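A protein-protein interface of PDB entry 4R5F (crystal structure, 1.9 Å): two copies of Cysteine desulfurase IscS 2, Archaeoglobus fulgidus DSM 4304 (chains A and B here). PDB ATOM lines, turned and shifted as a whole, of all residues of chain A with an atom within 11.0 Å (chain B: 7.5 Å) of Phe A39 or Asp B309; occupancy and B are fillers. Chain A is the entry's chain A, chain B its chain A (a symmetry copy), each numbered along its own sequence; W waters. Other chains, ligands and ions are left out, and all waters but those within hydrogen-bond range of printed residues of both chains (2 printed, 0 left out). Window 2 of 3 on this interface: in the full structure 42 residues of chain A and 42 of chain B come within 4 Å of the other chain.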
ATOM      1  N   TYR A  23       4.294  28.213   5.564  1.00  0.00           N
ATOM      2  CA  TYR A  23       5.320  29.096   5.037  1.00  0.00           C
ATOM      3  C   TYR A  23       5.155  30.555   5.490  1.00  0.00           C
ATOM      4  O   TYR A  23       6.044  31.386   5.248  1.00  0.00           O
ATOM      5  CB  TYR A  23       5.329  29.005   3.521  1.00  0.00           C
ATOM      6  CG  TYR A  23       5.791  27.623   3.104  1.00  0.00           C
ATOM      7  CD1 TYR A  23       7.135  27.315   3.110  1.00  0.00           C
ATOM      8  CD2 TYR A  23       4.884  26.617   2.783  1.00  0.00           C
ATOM      9  CE1 TYR A  23       7.600  26.066   2.775  1.00  0.00           C
ATOM     10  CE2 TYR A  23       5.333  25.338   2.429  1.00  0.00           C
ATOM     11  CZ  TYR A  23       6.710  25.078   2.444  1.00  0.00           C
ATOM     12  OH  TYR A  23       7.204  23.860   2.112  1.00  0.00           O
ATOM     13  N   SER A  27       8.004  28.179   8.486  1.00  0.00           N
ATOM     14  CA  SER A  27       9.081  28.029   7.534  1.00  0.00           C
ATOM     15  C   SER A  27       9.109  29.233   6.580  1.00  0.00           C
ATOM     16  O   SER A  27       8.715  29.117   5.415  1.00  0.00           O
ATOM     17  CB  SER A  27       8.904  26.699   6.773  1.00  0.00           C
ATOM     18  OG  SER A  27      10.022  26.442   5.948  1.00  0.00           O
ATOM     19  N   PHE A  28       9.616  30.366   7.082  1.00  0.00           N
ATOM     20  CA  PHE A  28       9.396  31.701   6.486  1.00  0.00           C
ATOM     21  C   PHE A  28      10.643  32.201   5.757  1.00  0.00           C
ATOM     22  O   PHE A  28      10.784  33.372   5.399  1.00  0.00           O
ATOM     23  CB  PHE A  28       8.954  32.686   7.609  1.00  0.00           C
ATOM     24  CG  PHE A  28       9.980  32.849   8.710  1.00  0.00           C
ATOM     25  CD1 PHE A  28      10.952  33.824   8.632  1.00  0.00           C
ATOM     26  CD2 PHE A  28       9.977  32.010   9.804  1.00  0.00           C
ATOM     27  CE1 PHE A  28      11.902  33.956   9.624  1.00  0.00           C
ATOM     28  CE2 PHE A  28      10.948  32.129  10.808  1.00  0.00           C
ATOM     29  CZ  PHE A  28      11.900  33.099  10.706  1.00  0.00           C
ATOM     30  N   GLY A  29      11.573  31.296   5.500  1.00  0.00           N
ATOM     31  CA  GLY A  29      12.830  31.703   4.908  1.00  0.00           C
ATOM     32  C   GLY A  29      12.733  32.328   3.535  1.00  0.00           C
ATOM     33  O   GLY A  29      11.766  32.127   2.792  1.00  0.00           O
ATOM     34  N   ASN A  30      13.756  33.118   3.228  1.00  0.00           N
ATOM     35  CA  ASN A  30      14.009  33.668   1.900  1.00  0.00           C
ATOM     36  C   ASN A  30      14.798  32.670   1.060  1.00  0.00           C
ATOM     37  O   ASN A  30      15.887  32.209   1.490  1.00  0.00           O
ATOM     38  CB  ASN A  30      14.770  34.990   2.039  1.00  0.00           C
ATOM     39  CG  ASN A  30      14.948  35.732   0.738  1.00  0.00           C
ATOM     40  OD1 ASN A  30      15.176  35.153  -0.325  1.00  0.00           O
ATOM     41  ND2 ASN A  30      14.866  37.057   0.822  1.00  0.00           N
ATOM     42  N   PRO A  31      14.265  32.300  -0.116  1.00  0.00           N
ATOM     43  CA  PRO A  31      14.973  31.284  -0.925  1.00  0.00           C
ATOM     44  C   PRO A  31      16.393  31.656  -1.327  1.00  0.00           C
ATOM     45  O   PRO A  31      17.164  30.788  -1.766  1.00  0.00           O
ATOM     46  CB  PRO A  31      14.107  31.172  -2.192  1.00  0.00           C
ATOM     47  CG  PRO A  31      12.759  31.592  -1.792  1.00  0.00           C
ATOM     48  CD  PRO A  31      12.990  32.704  -0.759  1.00  0.00           C
ATOM     49  N   SER A  32      16.739  32.931  -1.230  1.00  0.00           N
ATOM     50  CA  SER A  32      18.079  33.341  -1.622  1.00  0.00           C
ATOM     51  C   SER A  32      19.066  33.141  -0.469  1.00  0.00           C
ATOM     52  O   SER A  32      20.270  33.204  -0.689  1.00  0.00           O
ATOM     53  CB  SER A  32      18.092  34.805  -2.093  1.00  0.00           C
ATOM     54  OG  SER A  32      17.709  34.898  -3.468  1.00  0.00           O
ATOM     55  N   SER A  33      18.558  32.892   0.740  1.00  0.00           N
ATOM     56  CA  SER A  33      19.403  32.799   1.944  1.00  0.00           C
ATOM     57  C   SER A  33      20.145  31.450   1.936  1.00  0.00           C
ATOM     58  O   SER A  33      19.598  30.456   1.505  1.00  0.00           O
ATOM     59  CB  SER A  33      18.560  32.924   3.206  1.00  0.00           C
ATOM     60  OG  SER A  33      17.995  34.227   3.325  1.00  0.00           O
ATOM     61  N   VAL A  34      21.373  31.414   2.440  1.00  0.00           N
ATOM     62  CA  VAL A  34      22.196  30.214   2.346  1.00  0.00           C
ATOM     63  C   VAL A  34      22.310  29.567   3.718  1.00  0.00           C
ATOM     64  O   VAL A  34      23.387  29.430   4.303  1.00  0.00           O
ATOM     65  CB  VAL A  34      23.584  30.539   1.761  1.00  0.00           C
ATOM     66  CG1 VAL A  34      23.422  31.211   0.430  1.00  0.00           C
ATOM     67  CG2 VAL A  34      24.350  31.494   2.604  1.00  0.00           C
ATOM     68  N   HIS A  35      21.163  29.170   4.232  1.00  0.00           N
ATOM     69  CA  HIS A  35      21.094  28.440   5.481  1.00  0.00           C
ATOM     70  C   HIS A  35      19.847  27.589   5.390  1.00  0.00           C
ATOM     71  O   HIS A  35      19.096  27.666   4.410  1.00  0.00           O
ATOM     72  CB  HIS A  35      21.072  29.368   6.702  1.00  0.00           C
ATOM     73  CG  HIS A  35      20.081  30.483   6.599  1.00  0.00           C
ATOM     74  ND1 HIS A  35      18.725  30.261   6.490  1.00  0.00           N
ATOM     75  CD2 HIS A  35      20.247  31.830   6.573  1.00  0.00           C
ATOM     76  CE1 HIS A  35      18.098  31.425   6.383  1.00  0.00           C
ATOM     77  NE2 HIS A  35      18.995  32.393   6.436  1.00  0.00           N
ATOM     78  N   SER A  36      19.614  26.763   6.397  1.00  0.00           N
ATOM     79  CA  SER A  36      18.555  25.764   6.296  1.00  0.00           C
ATOM     80  C   SER A  36      17.165  26.354   6.010  1.00  0.00           C
ATOM     81  O   SER A  36      16.335  25.728   5.320  1.00  0.00           O
ATOM     82  CB  SER A  36      18.504  24.960   7.590  1.00  0.00           C
ATOM     83  OG  SER A  36      18.303  25.828   8.682  1.00  0.00           O
ATOM     84  N   TYR A  37      16.872  27.536   6.550  1.00  0.00           N
ATOM     85  CA  TYR A  37      15.561  28.150   6.290  1.00  0.00           C
ATOM     86  C   TYR A  37      15.485  28.556   4.825  1.00  0.00           C
ATOM     87  O   TYR A  37      14.449  28.382   4.166  1.00  0.00           O
ATOM     88  CB  TYR A  37      15.303  29.382   7.180  1.00  0.00           C
ATOM     89  CG  TYR A  37      14.757  29.068   8.556  1.00  0.00           C
ATOM     90  CD1 TYR A  37      15.523  28.411   9.494  1.00  0.00           C
ATOM     91  CD2 TYR A  37      13.478  29.452   8.920  1.00  0.00           C
ATOM     92  CE1 TYR A  37      15.027  28.120  10.751  1.00  0.00           C
ATOM     93  CE2 TYR A  37      12.973  29.162  10.167  1.00  0.00           C
ATOM     94  CZ  TYR A  37      13.752  28.514  11.080  1.00  0.00           C
ATOM     95  OH  TYR A  37      13.249  28.225  12.322  1.00  0.00           O
ATOM     96  N   GLY A  38      16.580  29.109   4.315  1.00  0.00           N
ATOM     97  CA  GLY A  38      16.659  29.440   2.913  1.00  0.00           C
ATOM     98  C   GLY A  38      16.438  28.199   2.034  1.00  0.00           C
ATOM     99  O   GLY A  38      15.721  28.242   1.031  1.00  0.00           O
ATOM    100  N   PHE A  39      17.091  27.094   2.388  1.00  0.00           N
ATOM    101  CA  PHE A  39      17.043  25.902   1.539  1.00  0.00           C
ATOM    102  C   PHE A  39      15.629  25.372   1.439  1.00  0.00           C
ATOM    103  O   PHE A  39      15.162  25.022   0.334  1.00  0.00           O
ATOM    104  CB  PHE A  39      17.940  24.785   2.081  1.00  0.00           C
ATOM    105  CG  PHE A  39      19.363  25.188   2.343  1.00  0.00           C
ATOM    106  CD1 PHE A  39      20.004  26.148   1.578  1.00  0.00           C
ATOM    107  CD2 PHE A  39      20.075  24.569   3.359  1.00  0.00           C
ATOM    108  CE1 PHE A  39      21.344  26.482   1.836  1.00  0.00           C
ATOM    109  CE2 PHE A  39      21.389  24.908   3.620  1.00  0.00           C
ATOM    110  CZ  PHE A  39      22.014  25.877   2.852  1.00  0.00           C
ATOM    111  N   LYS A  40      14.940  25.273   2.581  1.00  0.00           N
ATOM    112  CA  LYS A  40      13.565  24.779   2.550  1.00  0.00           C
ATOM    113  C   LYS A  40      12.673  25.664   1.686  1.00  0.00           C
ATOM    114  O   LYS A  40      11.840  25.155   0.939  1.00  0.00           O
ATOM    115  CB  LYS A  40      12.960  24.665   3.941  1.00  0.00           C
ATOM    116  CG  LYS A  40      13.601  23.619   4.836  1.00  0.00           C
ATOM    117  CD  LYS A  40      13.540  22.216   4.213  1.00  0.00           C
ATOM    118  N   ALA A  41      12.861  26.978   1.761  1.00  0.00           N
ATOM    119  CA  ALA A  41      12.058  27.903   0.966  1.00  0.00           C
ATOM    120  C   ALA A  41      12.315  27.696  -0.516  1.00  0.00           C
ATOM    121  O   ALA A  41      11.386  27.671  -1.329  1.00  0.00           O
ATOM    122  CB  ALA A  41      12.351  29.354   1.356  1.00  0.00           C
ATOM    123  N   ARG A  42      13.580  27.512  -0.864  1.00  0.00           N
ATOM    124  CA  ARG A  42      13.967  27.308  -2.250  1.00  0.00           C
ATOM    125  C   ARG A  42      13.367  26.010  -2.791  1.00  0.00           C
ATOM    126  O   ARG A  42      12.893  25.955  -3.930  1.00  0.00           O
ATOM    127  CB  ARG A  42      15.502  27.263  -2.377  1.00  0.00           C
ATOM    128  CG  ARG A  42      15.975  27.228  -3.828  1.00  0.00           C
ATOM    129  CD  ARG A  42      17.501  27.217  -3.965  1.00  0.00           C
ATOM    130  N   GLU A  43      13.352  24.982  -1.953  1.00  0.00           N
ATOM    131  CA  GLU A  43      12.815  23.677  -2.340  1.00  0.00           C
ATOM    132  C   GLU A  43      11.309  23.754  -2.551  1.00  0.00           C
ATOM    133  O   GLU A  43      10.749  23.126  -3.466  1.00  0.00           O
ATOM    134  CB  GLU A  43      13.150  22.633  -1.280  1.00  0.00           C
ATOM    135  CG  GLU A  43      12.359  21.351  -1.384  1.00  0.00           C
ATOM    136  CD  GLU A  43      12.879  20.298  -0.427  1.00  0.00           C
ATOM    137  OE1 GLU A  43      12.374  20.217   0.713  1.00  0.00           O
ATOM    138  OE2 GLU A  43      13.800  19.555  -0.814  1.00  0.00           O
ATOM    139  N   ALA A  44      10.646  24.521  -1.694  1.00  0.00           N
ATOM    140  CA  ALA A  44       9.220  24.726  -1.813  1.00  0.00           C
ATOM    141  C   ALA A  44       8.914  25.440  -3.117  1.00  0.00           C
ATOM    142  O   ALA A  44       7.978  25.087  -3.832  1.00  0.00           O
ATOM    143  CB  ALA A  44       8.684  25.525  -0.625  1.00  0.00           C
ATOM    144  N   VAL A  45       9.685  26.480  -3.418  1.00  0.00           N
ATOM    145  CA  VAL A  45       9.446  27.238  -4.634  1.00  0.00           C
ATOM    146  C   VAL A  45       9.653  26.385  -5.882  1.00  0.00           C
ATOM    147  O   VAL A  45       8.840  26.464  -6.846  1.00  0.00           O
ATOM    148  CB  VAL A  45      10.325  28.506  -4.687  1.00  0.00           C
ATOM    149  CG1 VAL A  45      10.306  29.166  -6.069  1.00  0.00           C
ATOM    150  CG2 VAL A  45       9.867  29.514  -3.617  1.00  0.00           C
ATOM    151  N   GLN A  46      10.724  25.586  -5.900  1.00  0.00           N
ATOM    152  CA  GLN A  46      11.051  24.754  -7.064  1.00  0.00           C
ATOM    153  C   GLN A  46       9.939  23.762  -7.324  1.00  0.00           C
ATOM    154  O   GLN A  46       9.538  23.526  -8.475  1.00  0.00           O
ATOM    155  CB  GLN A  46      12.384  23.992  -6.855  1.00  0.00           C
ATOM    156  CG  GLN A  46      13.663  24.879  -6.842  1.00  0.00           C
ATOM    157  CD  GLN A  46      14.930  24.164  -6.337  1.00  0.00           C
ATOM    158  OE1 GLN A  46      14.865  23.120  -5.682  1.00  0.00           O
ATOM    159  NE2 GLN A  46      16.090  24.742  -6.646  1.00  0.00           N
ATOM    160  N   GLU A  47       9.467  23.152  -6.249  1.00  0.00           N
ATOM    161  CA  GLU A  47       8.378  22.198  -6.321  1.00  0.00           C
ATOM    162  C   GLU A  47       7.168  22.859  -6.958  1.00  0.00           C
ATOM    163  O   GLU A  47       6.663  22.410  -8.006  1.00  0.00           O
ATOM    164  CB  GLU A  47       8.044  21.675  -4.924  1.00  0.00           C
ATOM    165  CG  GLU A  47       6.782  20.839  -4.870  1.00  0.00           C
ATOM    166  CD  GLU A  47       6.416  20.397  -3.475  1.00  0.00           C
ATOM    167  OE1 GLU A  47       6.185  19.187  -3.274  1.00  0.00           O
ATOM    168  OE2 GLU A  47       6.355  21.261  -2.574  1.00  0.00           O
ATOM    169  N   ALA A  48       6.728  23.949  -6.328  1.00  0.00           N
ATOM    170  CA  ALA A  48       5.563  24.689  -6.786  1.00  0.00           C
ATOM    171  C   ALA A  48       5.679  25.011  -8.262  1.00  0.00           C
ATOM    172  O   ALA A  48       4.720  24.866  -9.040  1.00  0.00           O
ATOM    173  CB  ALA A  48       5.383  25.980  -5.969  1.00  0.00           C
ATOM    174  N   GLU A 235      11.096  36.246  -3.063  1.00  0.00           N
ATOM    175  CA  GLU A 235       9.971  35.401  -3.439  1.00  0.00           C
ATOM    176  C   GLU A 235       8.869  35.422  -2.407  1.00  0.00           C
ATOM    177  O   GLU A 235       9.128  35.338  -1.225  1.00  0.00           O
ATOM    178  CB  GLU A 235      10.425  33.961  -3.675  1.00  0.00           C
ATOM    179  CG  GLU A 235      11.318  33.848  -4.833  1.00  0.00           C
ATOM    180  CD  GLU A 235      12.798  34.086  -4.531  1.00  0.00           C
ATOM    181  OE1 GLU A 235      13.159  34.669  -3.467  1.00  0.00           O
ATOM    182  OE2 GLU A 235      13.596  33.659  -5.395  1.00  0.00           O
ATOM    183  N   VAL A 237       6.921  33.234  -0.980  1.00  0.00           N
ATOM    184  CA  VAL A 237       6.916  31.783  -0.917  1.00  0.00           C
ATOM    185  C   VAL A 237       5.525  31.202  -0.579  1.00  0.00           C
ATOM    186  O   VAL A 237       5.105  30.230  -1.202  1.00  0.00           O
ATOM    187  CB  VAL A 237       7.952  31.286   0.091  1.00  0.00           C
ATOM    188  CG1 VAL A 237       7.928  29.788   0.140  1.00  0.00           C
ATOM    189  CG2 VAL A 237       9.376  31.806  -0.317  1.00  0.00           C
ATOM    190  N   VAL A 241       3.625  28.671  -3.113  1.00  0.00           N
ATOM    191  CA  VAL A 241       3.266  27.340  -2.691  1.00  0.00           C
ATOM    192  C   VAL A 241       1.758  27.096  -2.890  1.00  0.00           C
ATOM    193  O   VAL A 241       1.360  26.027  -3.307  1.00  0.00           O
ATOM    194  CB  VAL A 241       3.665  27.107  -1.236  1.00  0.00           C
ATOM    195  CG1 VAL A 241       3.031  25.861  -0.695  1.00  0.00           C
ATOM    196  CG2 VAL A 241       5.239  27.017  -1.106  1.00  0.00           C
ATOM    197  N   SER B 303      31.931  31.089   5.068  1.00  0.00           N
ATOM    198  CA  SER B 303      32.230  29.983   5.961  1.00  0.00           C
ATOM    199  C   SER B 303      31.722  30.199   7.376  1.00  0.00           C
ATOM    200  O   SER B 303      31.424  29.234   8.096  1.00  0.00           O
ATOM    201  CB  SER B 303      33.749  29.726   6.007  1.00  0.00           C
ATOM    202  OG  SER B 303      34.245  29.647   4.689  1.00  0.00           O
ATOM    203  N   ILE B 304      31.648  31.457   7.802  1.00  0.00           N
ATOM    204  CA  ILE B 304      31.044  31.733   9.086  1.00  0.00           C
ATOM    205  C   ILE B 304      29.590  31.322   8.990  1.00  0.00           C
ATOM    206  O   ILE B 304      29.058  30.611   9.853  1.00  0.00           O
ATOM    207  CB  ILE B 304      31.146  33.238   9.494  1.00  0.00           C
ATOM    208  CG1 ILE B 304      32.596  33.727   9.486  1.00  0.00           C
ATOM    209  CG2 ILE B 304      30.501  33.448  10.866  1.00  0.00           C
ATOM    210  CD1 ILE B 304      32.746  35.255   9.870  1.00  0.00           C
ATOM    211  N   VAL B 305      28.936  31.785   7.931  1.00  0.00           N
ATOM    212  CA  VAL B 305      27.521  31.512   7.758  1.00  0.00           C
ATOM    213  C   VAL B 305      27.285  30.010   7.685  1.00  0.00           C
ATOM    214  O   VAL B 305      26.305  29.518   8.242  1.00  0.00           O
ATOM    215  CB  VAL B 305      26.943  32.192   6.495  1.00  0.00           C
ATOM    216  CG1 VAL B 305      25.554  31.642   6.155  1.00  0.00           C
ATOM    217  CG2 VAL B 305      26.846  33.703   6.705  1.00  0.00           C
ATOM    218  N   LEU B 306      28.183  29.283   7.010  1.00  0.00           N
ATOM    219  CA  LEU B 306      28.039  27.846   6.916  1.00  0.00           C
ATOM    220  C   LEU B 306      28.179  27.237   8.293  1.00  0.00           C
ATOM    221  O   LEU B 306      27.338  26.445   8.724  1.00  0.00           O
ATOM    222  CB  LEU B 306      29.071  27.255   5.948  1.00  0.00           C
ATOM    223  CG  LEU B 306      29.357  25.743   5.990  1.00  0.00           C
ATOM    224  CD1 LEU B 306      28.184  24.893   5.513  1.00  0.00           C
ATOM    225  CD2 LEU B 306      30.575  25.451   5.149  1.00  0.00           C
ATOM    226  N   SER B 307      29.250  27.603   8.993  1.00  0.00           N
ATOM    227  CA  SER B 307      29.482  27.050  10.309  1.00  0.00           C
ATOM    228  C   SER B 307      28.319  27.346  11.255  1.00  0.00           C
ATOM    229  O   SER B 307      27.938  26.490  12.066  1.00  0.00           O
ATOM    230  CB  SER B 307      30.800  27.593  10.890  1.00  0.00           C
ATOM    231  OG  SER B 307      31.870  27.301  10.011  1.00  0.00           O
ATOM    232  N   LEU B 308      27.762  28.555  11.165  1.00  0.00           N
ATOM    233  CA  LEU B 308      26.664  28.916  12.023  1.00  0.00           C
ATOM    234  C   LEU B 308      25.423  28.083  11.706  1.00  0.00           C
ATOM    235  O   LEU B 308      24.737  27.613  12.616  1.00  0.00           O
ATOM    236  CB  LEU B 308      26.346  30.410  11.886  1.00  0.00           C
ATOM    237  CG  LEU B 308      27.378  31.342  12.534  1.00  0.00           C
ATOM    238  CD1 LEU B 308      26.918  32.737  12.357  1.00  0.00           C
ATOM    239  CD2 LEU B 308      27.592  31.033  14.004  1.00  0.00           C
ATOM    240  N   ASP B 309      25.152  27.879  10.415  1.00  0.00           N
ATOM    241  CA  ASP B 309      24.055  27.036   9.954  1.00  0.00           C
ATOM    242  C   ASP B 309      24.169  25.645  10.564  1.00  0.00           C
ATOM    243  O   ASP B 309      23.201  25.050  11.078  1.00  0.00           O
ATOM    244  CB  ASP B 309      24.093  26.962   8.419  1.00  0.00           C
ATOM    245  CG  ASP B 309      22.901  26.230   7.826  1.00  0.00           C
ATOM    246  OD1 ASP B 309      21.772  26.411   8.335  1.00  0.00           O
ATOM    247  OD2 ASP B 309      23.111  25.478   6.842  1.00  0.00           O
ATOM    248  N   MET B 310      25.388  25.107  10.490  1.00  0.00           N
ATOM    249  CA  MET B 310      25.605  23.766  10.987  1.00  0.00           C
ATOM    250  C   MET B 310      25.282  23.682  12.473  1.00  0.00           C
ATOM    251  O   MET B 310      24.881  22.620  12.952  1.00  0.00           O
ATOM    252  CB  MET B 310      27.034  23.318  10.732  1.00  0.00           C
ATOM    253  CG  MET B 310      27.330  22.980   9.275  1.00  0.00           C
ATOM    254  SD  MET B 310      29.093  22.663   9.062  1.00  0.00           S
ATOM    255  CE  MET B 310      29.106  21.714   7.557  1.00  0.00           C
ATOM    256  N   ALA B 311      25.473  24.790  13.196  1.00  0.00           N
ATOM    257  CA  ALA B 311      25.123  24.857  14.618  1.00  0.00           C
ATOM    258  C   ALA B 311      23.701  25.379  14.855  1.00  0.00           C
ATOM    259  O   ALA B 311      23.327  25.696  15.993  1.00  0.00           O
ATOM    260  CB  ALA B 311      26.129  25.744  15.371  1.00  0.00           C
ATOM    261  N   GLY B 312      22.916  25.511  13.792  1.00  0.00           N
ATOM    262  CA  GLY B 312      21.507  25.856  13.939  1.00  0.00           C
ATOM    263  C   GLY B 312      21.252  27.336  14.154  1.00  0.00           C
ATOM    264  O   GLY B 312      20.288  27.736  14.816  1.00  0.00           O
ATOM    265  N   ILE B 313      22.126  28.149  13.576  1.00  0.00           N
ATOM    266  CA  ILE B 313      22.021  29.595  13.665  1.00  0.00           C
ATOM    267  C   ILE B 313      22.015  30.146  12.257  1.00  0.00           C
ATOM    268  O   ILE B 313      22.936  29.867  11.484  1.00  0.00           O
ATOM    269  CB  ILE B 313      23.187  30.186  14.463  1.00  0.00           C
ATOM    270  CG1 ILE B 313      23.188  29.649  15.888  1.00  0.00           C
ATOM    271  CG2 ILE B 313      23.144  31.710  14.484  1.00  0.00           C
ATOM    272  CD1 ILE B 313      24.542  29.849  16.589  1.00  0.00           C
ATOM    273  N   GLN B 314      20.977  30.922  11.915  1.00  0.00           N
ATOM    274  CA  GLN B 314      20.872  31.493  10.580  1.00  0.00           C
ATOM    275  C   GLN B 314      21.289  32.939  10.532  1.00  0.00           C
ATOM    276  O   GLN B 314      20.793  33.778  11.278  1.00  0.00           O
ATOM    277  CB  GLN B 314      19.437  31.375  10.027  1.00  0.00           C
ATOM    278  CG  GLN B 314      18.932  29.944   9.957  1.00  0.00           C
ATOM    279  CD  GLN B 314      18.467  29.418  11.300  1.00  0.00           C
ATOM    280  OE1 GLN B 314      17.773  30.117  12.048  1.00  0.00           O
ATOM    281  NE2 GLN B 314      18.798  28.169  11.589  1.00  0.00           N
ATOM    282  N   ALA B 315      22.134  33.225   9.564  1.00  0.00           N
ATOM    283  CA  ALA B 315      22.755  34.517   9.416  1.00  0.00           C
ATOM    284  C   ALA B 315      23.039  34.716   7.947  1.00  0.00           C
ATOM    285  O   ALA B 315      22.728  33.870   7.123  1.00  0.00           O
ATOM    286  CB  ALA B 315      24.070  34.581  10.258  1.00  0.00           C
ATOM    287  N   VAL B 365      28.685  30.056  20.488  1.00  0.00           N
ATOM    288  CA  VAL B 365      29.163  29.360  19.305  1.00  0.00           C
ATOM    289  C   VAL B 365      30.191  30.151  18.513  1.00  0.00           C
ATOM    290  O   VAL B 365      31.214  29.612  18.077  1.00  0.00           O
ATOM    291  CB  VAL B 365      27.952  29.053  18.390  1.00  0.00           C
ATOM    292  CG1 VAL B 365      28.386  28.469  17.050  1.00  0.00           C
ATOM    293  CG2 VAL B 365      26.988  28.136  19.136  1.00  0.00           C
HETATM  294  O   HOH W   1      20.305  26.125  10.326  1.00  0.00           O
HETATM  295  O   HOH W   2      22.274  33.861   4.125  1.00  0.00           O
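The backbone NH (N) of Ser A36 lies within hydrogen-bond range of the side-chain carboxylate (OD1) of Asp B309 (2.9 Å).
The backbone NH (N) of Tyr A37 lies close to a ring nitrogen (ND1) of His A35, at 3.3 Å.
A ring nitrogen (ND1) of His A35 lies within hydrogen-bond range of the backbone NH (N) of Gly A38 (3.3 Å).
Among the printed residues, pairs that only touch across the chains: Val A34 with Val B305, His A35 with Asp B309, His A35 with Gln B314, His A35 with Ala B315, Ser A36 with Gln B314, Tyr A37 with Gln B314 and Phe A39 with Asp B309.
Of the printed residues of chain B, Phe A39 touches Asp B309.
Printed residues of chain A within 4 Å of Asp B309: His A35, Ser A36 and Phe A39.
No residue of chain B comes within 4 Å of Gly A38.
No residue of chain A comes within 4 Å of Ser B307.
No residue of chain A comes within 4 Å of Gly B312.
Of the printed residues of chain A, Val B305 touches Val A34.
Printed residues of chain B within 4 Å of Val A34: Val B305.
Printed residues of chain B within 4 Å of Ser A36: Asp B309 and Gln B314.
Ser A27 touches none of the printed residues of chain B.
The nearest printed residue of chain B that does not touch Phe A39 is Leu B306 (6.8 Å).
The nearest printed residue of chain A that does not touch Asp B309 is Val A34 (4.7 Å).
Of the 26 printed residues of chain A, 5 touch a printed residue of chain B.
Hydrophobic or aromatic side chains of chain A that line the printed part of chain B: Val A34, His A35, Tyr A37 and Phe A39.
Hydrophobic or aromatic side chains of chain B that line the printed part of chain A: Val B305.
Among the printed residues, 8 pairs touch across the chains.
Among the printed residues, no Asp or Glu carboxylate lies within 4 Å of a Lys or Arg side-chain nitrogen of the other chain.
No position is printed for both chains.
Water W1 lies within hydrogen-bond range of the side-chain carboxylate (OD1) of Asp B309, the side-chain hydroxyl (OG) of Ser A36 and the side-chain amide nitrogen (NE2) of Gln B314.
Water W2 bridges the backbone carbonyl oxygen (O) of Ala B315 and the backbone NH (N) of Val A34.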
